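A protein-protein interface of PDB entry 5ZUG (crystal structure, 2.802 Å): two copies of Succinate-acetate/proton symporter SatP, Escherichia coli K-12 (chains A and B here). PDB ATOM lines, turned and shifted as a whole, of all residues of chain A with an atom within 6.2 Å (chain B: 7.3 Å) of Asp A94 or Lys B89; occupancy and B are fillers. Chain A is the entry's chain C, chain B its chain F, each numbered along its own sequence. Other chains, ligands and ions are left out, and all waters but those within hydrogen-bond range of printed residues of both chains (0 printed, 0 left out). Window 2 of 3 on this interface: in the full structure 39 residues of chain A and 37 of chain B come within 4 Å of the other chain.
Hydrophobic or aromatic side chains of chain B within 4 Å of the printed part of chain A: Ile B39, Leu B41, Leu B86 and Leu B90. Among the printed residues, 11 pairs touch across the chains. Among the printed residues, Asp or Glu carboxylates within 4 Å of a Lys or Arg side-chain nitrogen of the other chain: Asp A94 with Lys B89 (3.7 Å).
The side-chain amino group (NZ) of Lys B89 lies within salt-bridge range of the side-chain carboxylate (OD1) of Asp A94, at 3.7 Å.
Positions printed for both chains: 84, 87, 88, 91, 92 and 93. Of the 11 pairs that touch across the chains among the printed residues, none has its exchanged pair printed and touching as well.
Of the printed residues of chain B, Ile A84 touches Gly B38 and Ile B39. Printed residues of chain B within 4 Å of Leu A92: Lys B89 (3.5 Å) and Leu B90 (3.9 Å). Asp A94 touches just one residue of chain B: Lys B89. Of the printed residues of chain A, Asp B37 touches Thr A93 and Pro A96. Of the printed residues of chain A, Gly B38 touches Ile A84 (3.5 Å) and Thr A93 (2.9 Å). Of the printed residues of chain A, Leu B41 touches Met A87 and Thr A93. Of the printed residues of chain A, Lys B89 touches Leu A92 and Asp A94. The nearest printed residue of chain B that does not touch Leu A92 is Leu B86 (4.04 Å).
O of Met A87 lies within hydrogen-bond range of N of Leu A92, at 2.9 Å. The side-chain sulfur (SD) of Met A87 is in hydrogen-bond range of the side-chain hydroxyl (OG1) of Thr A93. OD1 of Asp B37 sits at hydrogen-bond distance from N of Ile B39 (2.9 Å).
Among the printed residues, pairs that only touch across the chains: Ile A84 with Gly B38, Ile A84 with Ile B39, Met A87 with Leu B41, Met A87 with Leu B86, Leu A92 with Lys B89, Leu A92 with Leu B90, Thr A93 with Asp B37, Thr A93 with Gly B38, Thr A93 with Leu B41 and Pro A96 with Asp B37.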
ATOM      1  N   ILE A  84      12.427 -19.808 -23.972  1.00  0.00           N
ATOM      2  CA  ILE A  84      12.924 -20.726 -22.954  1.00  0.00           C
ATOM      3  C   ILE A  84      12.227 -22.074 -23.060  1.00  0.00           C
ATOM      4  O   ILE A  84      12.862 -23.124 -22.912  1.00  0.00           O
ATOM      5  CB  ILE A  84      12.754 -20.091 -21.561  1.00  0.00           C
ATOM      6  CG1 ILE A  84      13.861 -19.040 -21.329  1.00  0.00           C
ATOM      7  CG2 ILE A  84      12.634 -21.172 -20.461  1.00  0.00           C
ATOM      8  CD1 ILE A  84      13.518 -17.971 -20.294  1.00  0.00           C
ATOM      9  N   MET A  87      13.277 -23.490 -27.168  1.00  0.00           N
ATOM     10  CA  MET A  87      14.653 -23.819 -27.529  1.00  0.00           C
ATOM     11  C   MET A  87      15.076 -25.244 -27.137  1.00  0.00           C
ATOM     12  O   MET A  87      15.937 -25.811 -27.834  1.00  0.00           O
ATOM     13  CB  MET A  87      15.593 -22.784 -26.898  1.00  0.00           C
ATOM     14  CG  MET A  87      15.581 -21.441 -27.547  1.00  0.00           C
ATOM     15  SD  MET A  87      16.370 -20.310 -26.383  1.00  0.00           S
ATOM     16  CE  MET A  87      17.904 -19.947 -27.233  1.00  0.00           C
ATOM     17  N   PRO A  88      14.563 -25.857 -26.066  1.00  0.00           N
ATOM     18  CA  PRO A  88      14.850 -27.288 -25.876  1.00  0.00           C
ATOM     19  C   PRO A  88      14.287 -28.162 -26.989  1.00  0.00           C
ATOM     20  O   PRO A  88      15.052 -28.878 -27.647  1.00  0.00           O
ATOM     21  CB  PRO A  88      14.195 -27.586 -24.521  1.00  0.00           C
ATOM     22  CG  PRO A  88      14.220 -26.287 -23.815  1.00  0.00           C
ATOM     23  CD  PRO A  88      13.975 -25.258 -24.854  1.00  0.00           C
ATOM     24  N   GLY A  91      16.609 -28.305 -29.777  1.00  0.00           N
ATOM     25  CA  GLY A  91      17.993 -28.696 -29.582  1.00  0.00           C
ATOM     26  C   GLY A  91      18.977 -27.547 -29.494  1.00  0.00           C
ATOM     27  O   GLY A  91      20.129 -27.699 -29.918  1.00  0.00           O
ATOM     28  N   LEU A  92      18.582 -26.449 -28.884  1.00  0.00           N
ATOM     29  CA  LEU A  92      19.472 -25.334 -28.713  1.00  0.00           C
ATOM     30  C   LEU A  92      19.829 -25.115 -27.273  1.00  0.00           C
ATOM     31  O   LEU A  92      20.953 -24.955 -26.924  1.00  0.00           O
ATOM     32  CB  LEU A  92      18.776 -24.096 -29.158  1.00  0.00           C
ATOM     33  CG  LEU A  92      18.356 -24.067 -30.582  1.00  0.00           C
ATOM     34  CD1 LEU A  92      17.967 -22.649 -30.855  1.00  0.00           C
ATOM     35  CD2 LEU A  92      19.535 -24.441 -31.419  1.00  0.00           C
ATOM     36  N   THR A  93      18.787 -25.023 -26.457  1.00  0.00           N
ATOM     37  CA  THR A  93      18.929 -24.795 -25.035  1.00  0.00           C
ATOM     38  C   THR A  93      18.525 -26.100 -24.403  1.00  0.00           C
ATOM     39  O   THR A  93      17.621 -26.776 -24.895  1.00  0.00           O
ATOM     40  CB  THR A  93      17.998 -23.674 -24.540  1.00  0.00           C
ATOM     41  OG1 THR A  93      18.253 -22.476 -25.284  1.00  0.00           O
ATOM     42  CG2 THR A  93      18.227 -23.406 -23.061  1.00  0.00           C
ATOM     43  N   ASP A  94      19.189 -26.475 -23.323  1.00  0.00           N
ATOM     44  CA  ASP A  94      18.853 -27.730 -22.715  1.00  0.00           C
ATOM     45  C   ASP A  94      17.722 -27.144 -21.989  1.00  0.00           C
ATOM     46  O   ASP A  94      17.473 -25.971 -22.191  1.00  0.00           O
ATOM     47  CB  ASP A  94      19.916 -28.171 -21.753  1.00  0.00           C
ATOM     48  CG  ASP A  94      21.168 -28.597 -22.453  1.00  0.00           C
ATOM     49  OD1 ASP A  94      21.144 -28.825 -23.679  1.00  0.00           O
ATOM     50  OD2 ASP A  94      22.181 -28.725 -21.760  1.00  0.00           O
ATOM     51  N   ALA A  95      17.101 -27.937 -21.109  1.00  0.00           N
ATOM     52  CA  ALA A  95      15.954 -27.553 -20.277  1.00  0.00           C
ATOM     53  C   ALA A  95      16.409 -26.478 -19.307  1.00  0.00           C
ATOM     54  O   ALA A  95      17.609 -26.342 -19.068  1.00  0.00           O
ATOM     55  CB  ALA A  95      15.411 -28.757 -19.526  1.00  0.00           C
ATOM     56  N   PRO A  96      15.488 -25.679 -18.772  1.00  0.00           N
ATOM     57  CA  PRO A  96      15.961 -24.589 -17.939  1.00  0.00           C
ATOM     58  C   PRO A  96      16.067 -25.018 -16.483  1.00  0.00           C
ATOM     59  O   PRO A  96      15.426 -25.976 -16.172  1.00  0.00           O
ATOM     60  CB  PRO A  96      14.819 -23.607 -18.056  1.00  0.00           C
ATOM     61  CG  PRO A  96      13.592 -24.416 -18.207  1.00  0.00           C
ATOM     62  CD  PRO A  96      13.991 -25.819 -18.454  1.00  0.00           C
ATOM     63  N   LEU B  36      25.115 -21.480 -18.124  1.00  0.00           N
ATOM     64  CA  LEU B  36      24.673 -20.545 -19.154  1.00  0.00           C
ATOM     65  C   LEU B  36      23.454 -21.132 -19.860  1.00  0.00           C
ATOM     66  O   LEU B  36      23.564 -21.801 -20.895  1.00  0.00           O
ATOM     67  CB  LEU B  36      25.797 -20.225 -20.143  1.00  0.00           C
ATOM     68  CG  LEU B  36      25.727 -18.784 -20.667  1.00  0.00           C
ATOM     69  CD1 LEU B  36      27.067 -18.322 -21.256  1.00  0.00           C
ATOM     70  CD2 LEU B  36      24.557 -18.572 -21.650  1.00  0.00           C
ATOM     71  N   ASP B  37      22.286 -20.776 -19.337  1.00  0.00           N
ATOM     72  CA  ASP B  37      20.981 -21.365 -19.580  1.00  0.00           C
ATOM     73  C   ASP B  37      20.309 -20.707 -20.784  1.00  0.00           C
ATOM     74  O   ASP B  37      20.790 -19.714 -21.342  1.00  0.00           O
ATOM     75  CB  ASP B  37      20.131 -21.188 -18.316  1.00  0.00           C
ATOM     76  CG  ASP B  37      18.881 -22.043 -18.302  1.00  0.00           C
ATOM     77  OD1 ASP B  37      18.127 -22.060 -19.303  1.00  0.00           O
ATOM     78  OD2 ASP B  37      18.645 -22.704 -17.265  1.00  0.00           O
ATOM     79  N   GLY B  38      19.205 -21.318 -21.222  1.00  0.00           N
ATOM     80  CA  GLY B  38      18.300 -20.639 -22.125  1.00  0.00           C
ATOM     81  C   GLY B  38      17.621 -19.423 -21.515  1.00  0.00           C
ATOM     82  O   GLY B  38      17.179 -18.546 -22.260  1.00  0.00           O
ATOM     83  N   ILE B  39      17.521 -19.347 -20.179  1.00  0.00           N
ATOM     84  CA  ILE B  39      16.995 -18.136 -19.535  1.00  0.00           C
ATOM     85  C   ILE B  39      17.842 -16.926 -19.892  1.00  0.00           C
ATOM     86  O   ILE B  39      17.331 -15.869 -20.268  1.00  0.00           O
ATOM     87  CB  ILE B  39      16.921 -18.311 -18.013  1.00  0.00           C
ATOM     88  CG1 ILE B  39      15.807 -19.287 -17.649  1.00  0.00           C
ATOM     89  CG2 ILE B  39      16.823 -16.956 -17.343  1.00  0.00           C
ATOM     90  CD1 ILE B  39      15.745 -19.559 -16.198  1.00  0.00           C
ATOM     91  N   LEU B  41      19.872 -16.953 -22.441  1.00  0.00           N
ATOM     92  CA  LEU B  41      19.826 -16.876 -23.904  1.00  0.00           C
ATOM     93  C   LEU B  41      18.540 -16.223 -24.414  1.00  0.00           C
ATOM     94  O   LEU B  41      18.583 -15.427 -25.366  1.00  0.00           O
ATOM     95  CB  LEU B  41      19.999 -18.264 -24.519  1.00  0.00           C
ATOM     96  CG  LEU B  41      21.364 -18.923 -24.317  1.00  0.00           C
ATOM     97  CD1 LEU B  41      21.355 -20.337 -24.863  1.00  0.00           C
ATOM     98  CD2 LEU B  41      22.448 -18.082 -25.006  1.00  0.00           C
ATOM     99  N   ALA B  83      24.430 -15.050 -30.584  1.00  0.00           N
ATOM    100  CA  ALA B  83      24.744 -15.701 -31.855  1.00  0.00           C
ATOM    101  C   ALA B  83      26.015 -16.534 -31.742  1.00  0.00           C
ATOM    102  O   ALA B  83      26.112 -17.618 -32.327  1.00  0.00           O
ATOM    103  CB  ALA B  83      24.889 -14.665 -32.965  1.00  0.00           C
ATOM    104  N   ILE B  84      27.014 -16.025 -31.019  1.00  0.00           N
ATOM    105  CA  ILE B  84      28.247 -16.775 -30.780  1.00  0.00           C
ATOM    106  C   ILE B  84      27.972 -18.021 -29.944  1.00  0.00           C
ATOM    107  O   ILE B  84      28.597 -19.067 -30.151  1.00  0.00           O
ATOM    108  CB  ILE B  84      29.313 -15.866 -30.143  1.00  0.00           C
ATOM    109  CG1 ILE B  84      29.924 -14.954 -31.212  1.00  0.00           C
ATOM    110  CG2 ILE B  84      30.387 -16.693 -29.485  1.00  0.00           C
ATOM    111  CD1 ILE B  84      30.540 -13.708 -30.657  1.00  0.00           C
ATOM    112  N   LEU B  85      27.052 -17.932 -28.973  1.00  0.00           N
ATOM    113  CA  LEU B  85      26.727 -19.118 -28.181  1.00  0.00           C
ATOM    114  C   LEU B  85      25.798 -20.085 -28.918  1.00  0.00           C
ATOM    115  O   LEU B  85      25.812 -21.283 -28.615  1.00  0.00           O
ATOM    116  CB  LEU B  85      26.102 -18.740 -26.837  1.00  0.00           C
ATOM    117  CG  LEU B  85      26.943 -17.899 -25.878  1.00  0.00           C
ATOM    118  CD1 LEU B  85      26.167 -17.586 -24.592  1.00  0.00           C
ATOM    119  CD2 LEU B  85      28.279 -18.564 -25.581  1.00  0.00           C
ATOM    120  N   LEU B  86      24.971 -19.613 -29.863  1.00  0.00           N
ATOM    121  CA  LEU B  86      24.029 -20.518 -30.515  1.00  0.00           C
ATOM    122  C   LEU B  86      24.424 -20.945 -31.927  1.00  0.00           C
ATOM    123  O   LEU B  86      23.975 -22.005 -32.371  1.00  0.00           O
ATOM    124  CB  LEU B  86      22.617 -19.922 -30.578  1.00  0.00           C
ATOM    125  CG  LEU B  86      21.737 -19.935 -29.327  1.00  0.00           C
ATOM    126  CD1 LEU B  86      20.318 -19.559 -29.746  1.00  0.00           C
ATOM    127  CD2 LEU B  86      21.762 -21.294 -28.639  1.00  0.00           C
ATOM    128  N   MET B  87      25.258 -20.189 -32.643  1.00  0.00           N
ATOM    129  CA  MET B  87      25.695 -20.670 -33.951  1.00  0.00           C
ATOM    130  C   MET B  87      26.405 -22.020 -33.911  1.00  0.00           C
ATOM    131  O   MET B  87      26.379 -22.714 -34.945  1.00  0.00           O
ATOM    132  CB  MET B  87      26.602 -19.653 -34.653  1.00  0.00           C
ATOM    133  CG  MET B  87      25.906 -18.457 -35.256  1.00  0.00           C
ATOM    134  SD  MET B  87      27.130 -17.237 -35.746  1.00  0.00           S
ATOM    135  CE  MET B  87      27.051 -17.406 -37.519  1.00  0.00           C
ATOM    136  N   PRO B  88      27.112 -22.425 -32.813  1.00  0.00           N
ATOM    137  CA  PRO B  88      27.652 -23.792 -32.758  1.00  0.00           C
ATOM    138  C   PRO B  88      26.583 -24.872 -32.711  1.00  0.00           C
ATOM    139  O   PRO B  88      26.628 -25.833 -33.487  1.00  0.00           O
ATOM    140  CB  PRO B  88      28.470 -23.791 -31.463  1.00  0.00           C
ATOM    141  CG  PRO B  88      28.834 -22.379 -31.250  1.00  0.00           C
ATOM    142  CD  PRO B  88      27.652 -21.603 -31.712  1.00  0.00           C
ATOM    143  N   LYS B  89      25.600 -24.703 -31.816  1.00  0.00           N
ATOM    144  CA  LYS B  89      24.498 -25.656 -31.708  1.00  0.00           C
ATOM    145  C   LYS B  89      23.812 -25.901 -33.047  1.00  0.00           C
ATOM    146  O   LYS B  89      23.066 -26.870 -33.176  1.00  0.00           O
ATOM    147  CB  LYS B  89      23.476 -25.153 -30.676  1.00  0.00           C
ATOM    148  CG  LYS B  89      23.949 -25.122 -29.206  1.00  0.00           C
ATOM    149  CD  LYS B  89      23.781 -26.492 -28.531  1.00  0.00           C
ATOM    150  CE  LYS B  89      24.150 -26.472 -27.032  1.00  0.00           C
ATOM    151  NZ  LYS B  89      23.532 -27.605 -26.232  1.00  0.00           N
ATOM    152  N   LEU B  90      24.052 -25.049 -34.042  1.00  0.00           N
ATOM    153  CA  LEU B  90      23.499 -25.184 -35.384  1.00  0.00           C
ATOM    154  C   LEU B  90      24.502 -25.680 -36.426  1.00  0.00           C
ATOM    155  O   LEU B  90      24.142 -25.768 -37.610  1.00  0.00           O
ATOM    156  CB  LEU B  90      22.933 -23.836 -35.858  1.00  0.00           C
ATOM    157  CG  LEU B  90      21.856 -23.102 -35.063  1.00  0.00           C
ATOM    158  CD1 LEU B  90      21.821 -21.660 -35.551  1.00  0.00           C
ATOM    159  CD2 LEU B  90      20.489 -23.768 -35.172  1.00  0.00           C
ATOM    160  N   GLY B  91      25.754 -25.942 -36.045  1.00  0.00           N
ATOM    161  CA  GLY B  91      26.750 -26.344 -37.029  1.00  0.00           C
ATOM    162  C   GLY B  91      27.103 -25.280 -38.056  1.00  0.00           C
ATOM    163  O   GLY B  91      27.425 -25.611 -39.204  1.00  0.00           O
ATOM    164  N   LEU B  92      27.033 -24.002 -37.681  1.00  0.00           N
ATOM    165  CA  LEU B  92      27.458 -22.904 -38.546  1.00  0.00           C
ATOM    166  C   LEU B  92      28.859 -22.411 -38.221  1.00  0.00           C
ATOM    167  O   LEU B  92      29.621 -22.039 -39.126  1.00  0.00           O
ATOM    168  CB  LEU B  92      26.481 -21.732 -38.421  1.00  0.00           C
ATOM    169  CG  LEU B  92      25.025 -22.003 -38.757  1.00  0.00           C
ATOM    170  CD1 LEU B  92      24.174 -20.779 -38.420  1.00  0.00           C
ATOM    171  CD2 LEU B  92      24.960 -22.341 -40.232  1.00  0.00           C
ATOM    172  N   THR B  93      29.174 -22.392 -36.929  1.00  0.00           N
ATOM    173  CA  THR B  93      30.467 -21.934 -36.453  1.00  0.00           C
ATOM    174  C   THR B  93      30.963 -22.790 -35.294  1.00  0.00           C
ATOM    175  O   THR B  93      30.192 -23.220 -34.437  1.00  0.00           O
ATOM    176  CB  THR B  93      30.413 -20.462 -36.003  1.00  0.00           C
ATOM    177  OG1 THR B  93      29.642 -20.354 -34.800  1.00  0.00           O
ATOM    178  CG2 THR B  93      29.782 -19.598 -37.085  1.00  0.00           C
